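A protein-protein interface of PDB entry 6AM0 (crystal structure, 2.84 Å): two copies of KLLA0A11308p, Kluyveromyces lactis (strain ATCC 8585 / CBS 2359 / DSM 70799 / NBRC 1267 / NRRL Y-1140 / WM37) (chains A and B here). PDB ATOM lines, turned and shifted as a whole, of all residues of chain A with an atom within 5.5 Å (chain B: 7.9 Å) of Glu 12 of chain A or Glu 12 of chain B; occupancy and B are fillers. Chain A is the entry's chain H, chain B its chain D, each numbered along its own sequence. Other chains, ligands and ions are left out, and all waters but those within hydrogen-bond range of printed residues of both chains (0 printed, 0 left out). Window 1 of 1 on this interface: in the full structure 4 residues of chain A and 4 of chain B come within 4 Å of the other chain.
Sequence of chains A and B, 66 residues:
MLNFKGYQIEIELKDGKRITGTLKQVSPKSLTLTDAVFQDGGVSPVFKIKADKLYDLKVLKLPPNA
Leu 13 of chain A touches Arg 18 of chain B, but with the chains exchanged Arg 18 of chain A does not touch Leu 13 of chain B (6.5 Å). Arg 18 of chain A touches Asp 56 of chain B, but with the chains exchanged Asp 56 of chain A does not touch Arg 18 of chain B (4.9 Å). Tyr 55 of chain A touches Glu 10 of chain B, but with the chains exchanged Glu 10 of chain A does not touch Tyr 55 of chain B (9.6 Å). Tyr 55 of chain A touches Arg 18 of chain B, but with the chains exchanged Arg 18 of chain A does not touch Tyr 55 of chain B (4.7 Å). 11 positions are printed for both chains. Of the 7 pairs that touch across the chains among the printed residues, 3 have their exchanged pair printed and touching as well.
Among the printed residues, merely in contact across the chains: Tyr 55 of chain A with Arg 18 of chain B (2.8 Å) and Leu 13 of chain A with Arg 18 of chain B (3.7 Å).
OG1 of Thr 20 of chain B sits close to OE2 of Glu 10 of chain B (3.5 Å). O of Glu 10 of chain B lies within hydrogen-bond range of N of Lys 58 of chain B (2.9 Å). OE2 of Glu 12 of chain B is in salt-bridge range of NE of Arg 18 of chain B. The backbone carbonyl oxygen of Glu 12 of chain B lies within hydrogen-bond range of the backbone NH of Tyr 55 of chain B. The guanidinium group (NE) of Arg 18 of chain B lies close to the backbone carbonyl oxygen (O) of Gly 16 of chain B, at 3.5 Å. N of Glu 12 of chain A is in hydrogen-bond range of O of Asp 56 of chain A, 3.4 Å away.
Of chain B, only Glu 12 (3.3 Å) and Arg 18 (3.3 Å) come within 4 Å of Glu 12 of chain A. Of the printed residues of chain B, Leu 13 of chain A touches Arg 18 (3.7 Å). Of the printed residues of chain B, Arg 18 of chain A touches Glu 12 and Asp 56. Ile 19 of chain A touches none of the printed residues of chain B. Of the printed residues of chain B, Tyr 55 of chain A touches Glu 10 (3.1 Å) and Arg 18 (2.8 Å). Of chain A, only Glu 12 (3.3 Å) and Arg 18 (3.2 Å) come within 4 Å of Glu 12 of chain B. Of the printed residues of chain A, Arg 18 of chain B touches Glu 12, Leu 13 and Tyr 55. Of the printed residues of chain A, Asp 56 of chain B touches Arg 18. The nearest residue of chain B that does not touch Glu 12 of chain A is Asp 56 of chain B (5.3 Å). The nearest printed residue of chain A that does not touch Asp 56 of chain B is Glu 12 of chain A (5.3 Å).
OH of Tyr 55 of chain A sits at hydrogen-bond distance from OE2 of Glu 10 of chain B, 3.1 Å away. OE1 of Glu 12 of chain B lies within salt-bridge range of NH1 of Arg 18 of chain A (3.2 Å). The side-chain carboxylate (OE1) of Glu 12 of chain A is in salt-bridge range of the guanidinium group (NH1) of Arg 18 of chain B (3.3 Å). The side-chain carboxylate (OD2) of Asp 56 of chain B is in salt-bridge range of the guanidinium group (NH1) of Arg 18 of chain A (3.98 Å). The side-chain carboxylate (OE1) of Glu 12 of chain A lies close to the side-chain carboxylate (OE2) of Glu 12 of chain B, 3.3 Å away.
Of the 11 printed residues of chain A, 4 touch a printed residue of chain B. Along chain A the printed residues that touch a printed residue of chain B span positions 12 to 55. Printed residues of chain B that touch a printed residue of chain A: Glu 10, Glu 12, Arg 18 and Asp 56. Among the printed residues, 7 pairs touch across the chains. Among the printed residues, Asp or Glu carboxylates within 4 Å of a Lys or Arg side-chain nitrogen of the other chain: Glu 12 of chain A with Arg 18 of chain B (3.3 Å), Arg 18 of chain A with Glu 12 of chain B (3.2 Å) and Arg 18 of chain A with Asp 56 of chain B (3.98 Å).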
ATOM      1  N   GLU A  10      12.025  12.919   9.229  1.00  0.00           N
ATOM      2  CA  GLU A  10      12.410  14.127   9.945  1.00  0.00           C
ATOM      3  C   GLU A  10      11.698  14.168  11.293  1.00  0.00           C
ATOM      4  O   GLU A  10      10.506  13.861  11.377  1.00  0.00           O
ATOM      5  CB  GLU A  10      12.057  15.386   9.142  1.00  0.00           C
ATOM      6  CG  GLU A  10      11.606  15.113   7.720  1.00  0.00           C
ATOM      7  CD  GLU A  10      11.105  16.359   7.019  1.00  0.00           C
ATOM      8  OE1 GLU A  10      11.383  17.476   7.505  1.00  0.00           O
ATOM      9  OE2 GLU A  10      10.424  16.220   5.981  1.00  0.00           O
ATOM     10  N   ILE A  11      12.431  14.555  12.345  1.00  0.00           N
ATOM     11  CA  ILE A  11      11.884  14.747  13.686  1.00  0.00           C
ATOM     12  C   ILE A  11      12.279  16.123  14.216  1.00  0.00           C
ATOM     13  O   ILE A  11      13.217  16.759  13.722  1.00  0.00           O
ATOM     14  CB  ILE A  11      12.323  13.648  14.675  1.00  0.00           C
ATOM     15  CG1 ILE A  11      13.843  13.638  14.854  1.00  0.00           C
ATOM     16  CG2 ILE A  11      11.806  12.290  14.220  1.00  0.00           C
ATOM     17  CD1 ILE A  11      14.317  14.383  16.095  1.00  0.00           C
ATOM     18  N   GLU A  12      11.550  16.579  15.251  1.00  0.00           N
ATOM     19  CA  GLU A  12      11.699  17.951  15.716  1.00  0.00           C
ATOM     20  C   GLU A  12      11.717  18.099  17.246  1.00  0.00           C
ATOM     21  O   GLU A  12      11.402  17.184  18.023  1.00  0.00           O
ATOM     22  CB  GLU A  12      10.575  18.792  15.100  1.00  0.00           C
ATOM     23  CG  GLU A  12      10.434  18.595  13.575  1.00  0.00           C
ATOM     24  CD  GLU A  12       9.453  19.549  12.962  1.00  0.00           C
ATOM     25  OE1 GLU A  12       9.110  20.532  13.637  1.00  0.00           O
ATOM     26  OE2 GLU A  12       8.872  19.286  11.896  1.00  0.00           O
ATOM     27  N   LEU A  13      12.155  19.284  17.651  1.00  0.00           N
ATOM     28  CA  LEU A  13      11.943  19.793  18.980  1.00  0.00           C
ATOM     29  C   LEU A  13      11.891  21.328  18.918  1.00  0.00           C
ATOM     30  O   LEU A  13      12.684  21.977  18.227  1.00  0.00           O
ATOM     31  CB  LEU A  13      13.039  19.284  19.903  1.00  0.00           C
ATOM     32  CG  LEU A  13      13.059  19.749  21.353  1.00  0.00           C
ATOM     33  CD1 LEU A  13      13.911  21.003  21.485  1.00  0.00           C
ATOM     34  CD2 LEU A  13      11.653  19.965  21.915  1.00  0.00           C
ATOM     35  N   LYS A  17      15.533  21.793  17.679  1.00  0.00           N
ATOM     36  CA  LYS A  17      16.467  21.045  16.848  1.00  0.00           C
ATOM     37  C   LYS A  17      15.722  19.997  16.012  1.00  0.00           C
ATOM     38  O   LYS A  17      14.837  19.313  16.533  1.00  0.00           O
ATOM     39  CB  LYS A  17      17.553  20.382  17.714  1.00  0.00           C
ATOM     40  CG  LYS A  17      18.169  21.286  18.783  1.00  0.00           C
ATOM     41  CD  LYS A  17      18.720  22.583  18.203  1.00  0.00           C
ATOM     42  CE  LYS A  17      19.269  23.463  19.312  1.00  0.00           C
ATOM     43  NZ  LYS A  17      19.725  24.781  18.806  1.00  0.00           N
ATOM     44  N   ARG A  18      16.128  19.848  14.740  1.00  0.00           N
ATOM     45  CA  ARG A  18      15.499  18.942  13.783  1.00  0.00           C
ATOM     46  C   ARG A  18      16.516  17.905  13.307  1.00  0.00           C
ATOM     47  O   ARG A  18      17.652  18.248  12.962  1.00  0.00           O
ATOM     48  CB  ARG A  18      14.938  19.675  12.551  1.00  0.00           C
ATOM     49  CG  ARG A  18      13.905  20.767  12.734  1.00  0.00           C
ATOM     50  CD  ARG A  18      13.197  21.023  11.405  1.00  0.00           C
ATOM     51  NE  ARG A  18      12.176  22.087  11.474  1.00  0.00           N
ATOM     52  CZ  ARG A  18      11.295  22.312  10.501  1.00  0.00           C
ATOM     53  NH1 ARG A  18      10.357  23.260  10.630  1.00  0.00           N
ATOM     54  NH2 ARG A  18      11.373  21.595   9.396  1.00  0.00           N
ATOM     55  N   ILE A  19      16.119  16.625  13.303  1.00  0.00           N
ATOM     56  CA  ILE A  19      16.995  15.535  12.863  1.00  0.00           C
ATOM     57  C   ILE A  19      16.389  14.889  11.624  1.00  0.00           C
ATOM     58  O   ILE A  19      15.182  14.634  11.571  1.00  0.00           O
ATOM     59  CB  ILE A  19      17.265  14.469  13.957  1.00  0.00           C
ATOM     60  CG1 ILE A  19      17.874  15.079  15.227  1.00  0.00           C
ATOM     61  CG2 ILE A  19      18.192  13.345  13.436  1.00  0.00           C
ATOM     62  CD1 ILE A  19      18.966  16.117  14.968  1.00  0.00           C
ATOM     63  N   LYS A  53      11.239  12.533  23.455  1.00  0.00           N
ATOM     64  CA  LYS A  53      11.899  13.752  23.009  1.00  0.00           C
ATOM     65  C   LYS A  53      11.418  14.214  21.639  1.00  0.00           C
ATOM     66  O   LYS A  53      12.000  15.142  21.068  1.00  0.00           O
ATOM     67  CB  LYS A  53      13.419  13.558  22.974  1.00  0.00           C
ATOM     68  CG  LYS A  53      14.010  12.892  24.210  1.00  0.00           C
ATOM     69  CD  LYS A  53      14.177  13.906  25.336  1.00  0.00           C
ATOM     70  CE  LYS A  53      14.982  13.343  26.496  1.00  0.00           C
ATOM     71  NZ  LYS A  53      15.466  14.418  27.409  1.00  0.00           N
ATOM     72  N   LEU A  54      10.376  13.589  21.102  1.00  0.00           N
ATOM     73  CA  LEU A  54       9.851  13.922  19.785  1.00  0.00           C
ATOM     74  C   LEU A  54       8.563  14.712  19.960  1.00  0.00           C
ATOM     75  O   LEU A  54       7.603  14.213  20.551  1.00  0.00           O
ATOM     76  CB  LEU A  54       9.588  12.659  18.965  1.00  0.00           C
ATOM     77  CG  LEU A  54      10.779  11.791  18.567  1.00  0.00           C
ATOM     78  CD1 LEU A  54      10.375  10.903  17.407  1.00  0.00           C
ATOM     79  CD2 LEU A  54      11.971  12.651  18.205  1.00  0.00           C
ATOM     80  N   TYR A  55       8.536  15.941  19.452  1.00  0.00           N
ATOM     81  CA  TYR A  55       7.252  16.622  19.346  1.00  0.00           C
ATOM     82  C   TYR A  55       6.469  16.111  18.143  1.00  0.00           C
ATOM     83  O   TYR A  55       5.282  15.785  18.261  1.00  0.00           O
ATOM     84  CB  TYR A  55       7.447  18.134  19.253  1.00  0.00           C
ATOM     85  CG  TYR A  55       6.164  18.930  19.374  1.00  0.00           C
ATOM     86  CD1 TYR A  55       5.168  18.864  18.392  1.00  0.00           C
ATOM     87  CD2 TYR A  55       5.948  19.768  20.459  1.00  0.00           C
ATOM     88  CE1 TYR A  55       4.015  19.612  18.503  1.00  0.00           C
ATOM     89  CE2 TYR A  55       4.798  20.502  20.568  1.00  0.00           C
ATOM     90  CZ  TYR A  55       3.818  20.440  19.603  1.00  0.00           C
ATOM     91  OH  TYR A  55       2.703  21.172  19.733  1.00  0.00           O
ATOM     92  N   ASP A  56       7.110  16.039  16.978  1.00  0.00           N
ATOM     93  CA  ASP A  56       6.390  15.700  15.761  1.00  0.00           C
ATOM     94  C   ASP A  56       7.311  14.960  14.800  1.00  0.00           C
ATOM     95  O   ASP A  56       8.539  15.033  14.896  1.00  0.00           O
ATOM     96  CB  ASP A  56       5.803  16.947  15.084  1.00  0.00           C
ATOM     97  CG  ASP A  56       4.865  16.601  13.934  1.00  0.00           C
ATOM     98  OD1 ASP A  56       4.801  15.410  13.559  1.00  0.00           O
ATOM     99  OD2 ASP A  56       4.189  17.513  13.411  1.00  0.00           O
ATOM    100  N   ILE B   9      -4.237  27.519  14.309  1.00  0.00           N
ATOM    101  CA  ILE B   9      -2.975  27.588  13.579  1.00  0.00           C
ATOM    102  C   ILE B   9      -1.813  27.516  14.562  1.00  0.00           C
ATOM    103  O   ILE B   9      -1.893  28.050  15.676  1.00  0.00           O
ATOM    104  CB  ILE B   9      -2.889  28.875  12.727  1.00  0.00           C
ATOM    105  CG1 ILE B   9      -4.086  28.978  11.779  1.00  0.00           C
ATOM    106  CG2 ILE B   9      -1.587  28.936  11.937  1.00  0.00           C
ATOM    107  CD1 ILE B   9      -4.250  27.786  10.865  1.00  0.00           C
ATOM    108  N   GLU B  10      -0.735  26.846  14.145  1.00  0.00           N
ATOM    109  CA  GLU B  10       0.516  26.784  14.892  1.00  0.00           C
ATOM    110  C   GLU B  10       1.668  27.032  13.928  1.00  0.00           C
ATOM    111  O   GLU B  10       1.761  26.377  12.886  1.00  0.00           O
ATOM    112  CB  GLU B  10       0.670  25.429  15.590  1.00  0.00           C
ATOM    113  CG  GLU B  10       1.638  25.423  16.761  1.00  0.00           C
ATOM    114  CD  GLU B  10       1.452  24.212  17.656  1.00  0.00           C
ATOM    115  OE1 GLU B  10       0.529  23.411  17.389  1.00  0.00           O
ATOM    116  OE2 GLU B  10       2.224  24.063  18.628  1.00  0.00           O
ATOM    117  N   ILE B  11       2.540  27.980  14.278  1.00  0.00           N
ATOM    118  CA  ILE B  11       3.619  28.448  13.419  1.00  0.00           C
ATOM    119  C   ILE B  11       4.931  28.324  14.182  1.00  0.00           C
ATOM    120  O   ILE B  11       4.951  28.196  15.407  1.00  0.00           O
ATOM    121  CB  ILE B  11       3.391  29.901  12.930  1.00  0.00           C
ATOM    122  CG1 ILE B  11       3.324  30.889  14.102  1.00  0.00           C
ATOM    123  CG2 ILE B  11       2.118  29.997  12.106  1.00  0.00           C
ATOM    124  CD1 ILE B  11       4.607  31.662  14.353  1.00  0.00           C
ATOM    125  N   GLU B  12       6.037  28.374  13.444  1.00  0.00           N
ATOM    126  CA  GLU B  12       7.356  28.172  14.028  1.00  0.00           C
ATOM    127  C   GLU B  12       8.290  29.276  13.569  1.00  0.00           C
ATOM    128  O   GLU B  12       8.170  29.762  12.443  1.00  0.00           O
ATOM    129  CB  GLU B  12       7.955  26.825  13.618  1.00  0.00           C
ATOM    130  CG  GLU B  12       7.118  25.620  13.977  1.00  0.00           C
ATOM    131  CD  GLU B  12       7.855  24.322  13.733  1.00  0.00           C
ATOM    132  OE1 GLU B  12       9.029  24.378  13.294  1.00  0.00           O
ATOM    133  OE2 GLU B  12       7.298  23.256  14.079  1.00  0.00           O
ATOM    134  N   LEU B  13       9.228  29.657  14.439  1.00  0.00           N
ATOM    135  CA  LEU B  13      10.224  30.676  14.141  1.00  0.00           C
ATOM    136  C   LEU B  13      11.596  30.010  13.939  1.00  0.00           C
ATOM    137  O   LEU B  13      11.680  28.793  13.714  1.00  0.00           O
ATOM    138  CB  LEU B  13      10.213  31.726  15.255  1.00  0.00           C
ATOM    139  CG  LEU B  13       8.854  32.377  15.556  1.00  0.00           C
ATOM    140  CD1 LEU B  13       9.032  33.558  16.489  1.00  0.00           C
ATOM    141  CD2 LEU B  13       8.121  32.804  14.291  1.00  0.00           C
ATOM    142  N   LYS B  14      12.673  30.804  14.019  1.00  0.00           N
ATOM    143  CA  LYS B  14      13.977  30.295  13.593  1.00  0.00           C
ATOM    144  C   LYS B  14      14.526  29.231  14.538  1.00  0.00           C
ATOM    145  O   LYS B  14      15.239  28.325  14.092  1.00  0.00           O
ATOM    146  CB  LYS B  14      14.983  31.442  13.439  1.00  0.00           C
ATOM    147  CG  LYS B  14      15.483  32.046  14.739  1.00  0.00           C
ATOM    148  CD  LYS B  14      16.545  33.114  14.499  1.00  0.00           C
ATOM    149  CE  LYS B  14      17.125  33.619  15.813  1.00  0.00           C
ATOM    150  NZ  LYS B  14      18.154  34.676  15.613  1.00  0.00           N
ATOM    151  N   ASP B  15      14.211  29.304  15.831  1.00  0.00           N
ATOM    152  CA  ASP B  15      14.756  28.367  16.805  1.00  0.00           C
ATOM    153  C   ASP B  15      13.756  27.284  17.188  1.00  0.00           C
ATOM    154  O   ASP B  15      13.758  26.811  18.331  1.00  0.00           O
ATOM    155  CB  ASP B  15      15.237  29.116  18.047  1.00  0.00           C
ATOM    156  CG  ASP B  15      16.071  30.334  17.705  1.00  0.00           C
ATOM    157  OD1 ASP B  15      17.260  30.168  17.355  1.00  0.00           O
ATOM    158  OD2 ASP B  15      15.533  31.459  17.780  1.00  0.00           O
ATOM    159  N   GLY B  16      12.898  26.882  16.254  1.00  0.00           N
ATOM    160  CA  GLY B  16      11.844  25.944  16.574  1.00  0.00           C
ATOM    161  C   GLY B  16      10.806  26.440  17.557  1.00  0.00           C
ATOM    162  O   GLY B  16       9.954  25.657  17.978  1.00  0.00           O
ATOM    163  N   LYS B  17      10.844  27.710  17.942  1.00  0.00           N
ATOM    164  CA  LYS B  17       9.813  28.252  18.817  1.00  0.00           C
ATOM    165  C   LYS B  17       8.474  28.304  18.078  1.00  0.00           C
ATOM    166  O   LYS B  17       8.412  28.703  16.913  1.00  0.00           O
ATOM    167  CB  LYS B  17      10.242  29.630  19.313  1.00  0.00           C
ATOM    168  CG  LYS B  17      11.693  29.638  19.776  1.00  0.00           C
ATOM    169  CD  LYS B  17      11.911  28.523  20.798  1.00  0.00           C
ATOM    170  CE  LYS B  17      13.343  28.461  21.249  1.00  0.00           C
ATOM    171  NZ  LYS B  17      13.642  29.747  21.924  1.00  0.00           N
ATOM    172  N   ARG B  18       7.385  27.953  18.784  1.00  0.00           N
ATOM    173  CA  ARG B  18       6.065  27.755  18.185  1.00  0.00           C
ATOM    174  C   ARG B  18       5.037  28.689  18.808  1.00  0.00           C
ATOM    175  O   ARG B  18       4.979  28.835  20.033  1.00  0.00           O
ATOM    176  CB  ARG B  18       5.617  26.301  18.392  1.00  0.00           C
ATOM    177  CG  ARG B  18       6.702  25.347  17.908  1.00  0.00           C
ATOM    178  CD  ARG B  18       6.454  23.851  18.054  1.00  0.00           C
ATOM    179  NE  ARG B  18       7.623  23.145  17.528  1.00  0.00           N
ATOM    180  CZ  ARG B  18       7.687  21.842  17.306  1.00  0.00           C
ATOM    181  NH1 ARG B  18       8.798  21.311  16.824  1.00  0.00           N
ATOM    182  NH2 ARG B  18       6.632  21.089  17.551  1.00  0.00           N
ATOM    183  N   ILE B  19       4.227  29.319  17.957  1.00  0.00           N
ATOM    184  CA  ILE B  19       3.154  30.205  18.388  1.00  0.00           C
ATOM    185  C   ILE B  19       1.852  29.557  17.947  1.00  0.00           C
ATOM    186  O   ILE B  19       1.745  29.081  16.813  1.00  0.00           O
ATOM    187  CB  ILE B  19       3.283  31.628  17.799  1.00  0.00           C
ATOM    188  CG1 ILE B  19       4.660  32.233  18.091  1.00  0.00           C
ATOM    189  CG2 ILE B  19       2.167  32.517  18.320  1.00  0.00           C
ATOM    190  CD1 ILE B  19       5.178  31.980  19.489  1.00  0.00           C
ATOM    191  N   THR B  20       0.864  29.542  18.832  1.00  0.00           N
ATOM    192  CA  THR B  20      -0.435  28.959  18.530  1.00  0.00           C
ATOM    193  C   THR B  20      -1.506  30.026  18.681  1.00  0.00           C
ATOM    194  O   THR B  20      -1.499  30.784  19.654  1.00  0.00           O
ATOM    195  CB  THR B  20      -0.753  27.781  19.464  1.00  0.00           C
ATOM    196  OG1 THR B  20       0.352  26.868  19.498  1.00  0.00           O
ATOM    197  CG2 THR B  20      -1.993  27.041  18.989  1.00  0.00           C
ATOM    198  N   GLN B  39       5.087  29.096  23.120  1.00  0.00           N
ATOM    199  CA  GLN B  39       5.722  27.912  23.696  1.00  0.00           C
ATOM    200  C   GLN B  39       6.562  28.267  24.917  1.00  0.00           C
ATOM    201  O   GLN B  39       6.491  27.594  25.952  1.00  0.00           O
ATOM    202  CB  GLN B  39       6.585  27.209  22.647  1.00  0.00           C
ATOM    203  CG  GLN B  39       7.158  25.872  23.114  1.00  0.00           C
ATOM    204  CD  GLN B  39       7.666  25.013  21.971  1.00  0.00           C
ATOM    205  OE1 GLN B  39       7.796  25.483  20.843  1.00  0.00           O
ATOM    206  NE2 GLN B  39       7.945  23.746  22.257  1.00  0.00           N
ATOM    207  N   ILE B  49       2.270  39.054  12.533  1.00  0.00           N
ATOM    208  CA  ILE B  49       3.558  38.491  12.143  1.00  0.00           C
ATOM    209  C   ILE B  49       3.709  38.586  10.630  1.00  0.00           C
ATOM    210  O   ILE B  49       2.725  38.577   9.887  1.00  0.00           O
ATOM    211  CB  ILE B  49       3.688  37.022  12.622  1.00  0.00           C
ATOM    212  CG1 ILE B  49       5.067  36.437  12.303  1.00  0.00           C
ATOM    213  CG2 ILE B  49       2.601  36.160  12.002  1.00  0.00           C
ATOM    214  CD1 ILE B  49       6.205  37.099  13.026  1.00  0.00           C
ATOM    215  N   LYS B  53       9.459  36.003   8.626  1.00  0.00           N
ATOM    216  CA  LYS B  53       9.993  35.381   9.827  1.00  0.00           C
ATOM    217  C   LYS B  53       9.443  33.980  10.080  1.00  0.00           C
ATOM    218  O   LYS B  53       9.717  33.407  11.138  1.00  0.00           O
ATOM    219  CB  LYS B  53       9.700  36.269  11.039  1.00  0.00           C
ATOM    220  CG  LYS B  53       9.955  37.750  10.799  1.00  0.00           C
ATOM    221  CD  LYS B  53      11.425  38.112  10.915  1.00  0.00           C
ATOM    222  CE  LYS B  53      11.600  39.623  10.900  1.00  0.00           C
ATOM    223  NZ  LYS B  53      12.943  40.052  11.376  1.00  0.00           N
ATOM    224  N   LEU B  54       8.711  33.403   9.130  1.00  0.00           N
ATOM    225  CA  LEU B  54       8.068  32.108   9.323  1.00  0.00           C
ATOM    226  C   LEU B  54       8.862  31.009   8.632  1.00  0.00           C
ATOM    227  O   LEU B  54       9.150  31.100   7.434  1.00  0.00           O
ATOM    228  CB  LEU B  54       6.636  32.121   8.788  1.00  0.00           C
ATOM    229  CG  LEU B  54       5.645  33.032   9.508  1.00  0.00           C
ATOM    230  CD1 LEU B  54       4.223  32.603   9.193  1.00  0.00           C
ATOM    231  CD2 LEU B  54       5.899  33.016  11.006  1.00  0.00           C
ATOM    232  N   TYR B  55       9.194  29.964   9.388  1.00  0.00           N
ATOM    233  CA  TYR B  55       9.929  28.826   8.854  1.00  0.00           C
ATOM    234  C   TYR B  55       9.050  27.614   8.577  1.00  0.00           C
ATOM    235  O   TYR B  55       9.370  26.832   7.676  1.00  0.00           O
ATOM    236  CB  TYR B  55      11.066  28.441   9.807  1.00  0.00           C
ATOM    237  CG  TYR B  55      12.229  29.407   9.748  1.00  0.00           C
ATOM    238  CD1 TYR B  55      12.201  30.602  10.455  1.00  0.00           C
ATOM    239  CD2 TYR B  55      13.347  29.132   8.971  1.00  0.00           C
ATOM    240  CE1 TYR B  55      13.261  31.492  10.393  1.00  0.00           C
ATOM    241  CE2 TYR B  55      14.410  30.014   8.907  1.00  0.00           C
ATOM    242  CZ  TYR B  55      14.362  31.191   9.620  1.00  0.00           C
ATOM    243  OH  TYR B  55      15.418  32.072   9.558  1.00  0.00           O
ATOM    244  N   ASP B  56       7.953  27.434   9.315  1.00  0.00           N
ATOM    245  CA  ASP B  56       6.963  26.433   8.940  1.00  0.00           C
ATOM    246  C   ASP B  56       5.653  26.757   9.647  1.00  0.00           C
ATOM    247  O   ASP B  56       5.641  27.401  10.702  1.00  0.00           O
ATOM    248  CB  ASP B  56       7.436  25.014   9.296  1.00  0.00           C
ATOM    249  CG  ASP B  56       6.543  23.919   8.716  1.00  0.00           C
ATOM    250  OD1 ASP B  56       5.326  24.138   8.539  1.00  0.00           O
ATOM    251  OD2 ASP B  56       7.069  22.823   8.431  1.00  0.00           O
ATOM    252  N   LEU B  57       4.554  26.297   9.047  1.00  0.00           N
ATOM    253  CA  LEU B  57       3.205  26.522   9.545  1.00  0.00           C
ATOM    254  C   LEU B  57       2.412  25.229   9.403  1.00  0.00           C
ATOM    255  O   LEU B  57       2.509  24.549   8.379  1.00  0.00           O
ATOM    256  CB  LEU B  57       2.527  27.670   8.778  1.00  0.00           C
ATOM    257  CG  LEU B  57       1.035  27.975   8.942  1.00  0.00           C
ATOM    258  CD1 LEU B  57       0.807  29.467   8.800  1.00  0.00           C
ATOM    259  CD2 LEU B  57       0.191  27.226   7.920  1.00  0.00           C
ATOM    260  N   LYS B  58       1.614  24.899  10.418  1.00  0.00           N
ATOM    261  CA  LYS B  58       0.741  23.737  10.329  1.00  0.00           C
ATOM    262  C   LYS B  58      -0.548  24.054  11.082  1.00  0.00           C
ATOM    263  O   LYS B  58      -0.574  24.918  11.963  1.00  0.00           O
ATOM    264  CB  LYS B  58       1.455  22.477  10.844  1.00  0.00           C
ATOM    265  CG  LYS B  58       0.990  21.181  10.184  1.00  0.00           C
ATOM    266  CD  LYS B  58       1.099  19.973  11.096  1.00  0.00           C
ATOM    267  CE  LYS B  58       0.396  18.768  10.487  1.00  0.00           C
ATOM    268  NZ  LYS B  58       0.626  17.533  11.282  1.00  0.00           N
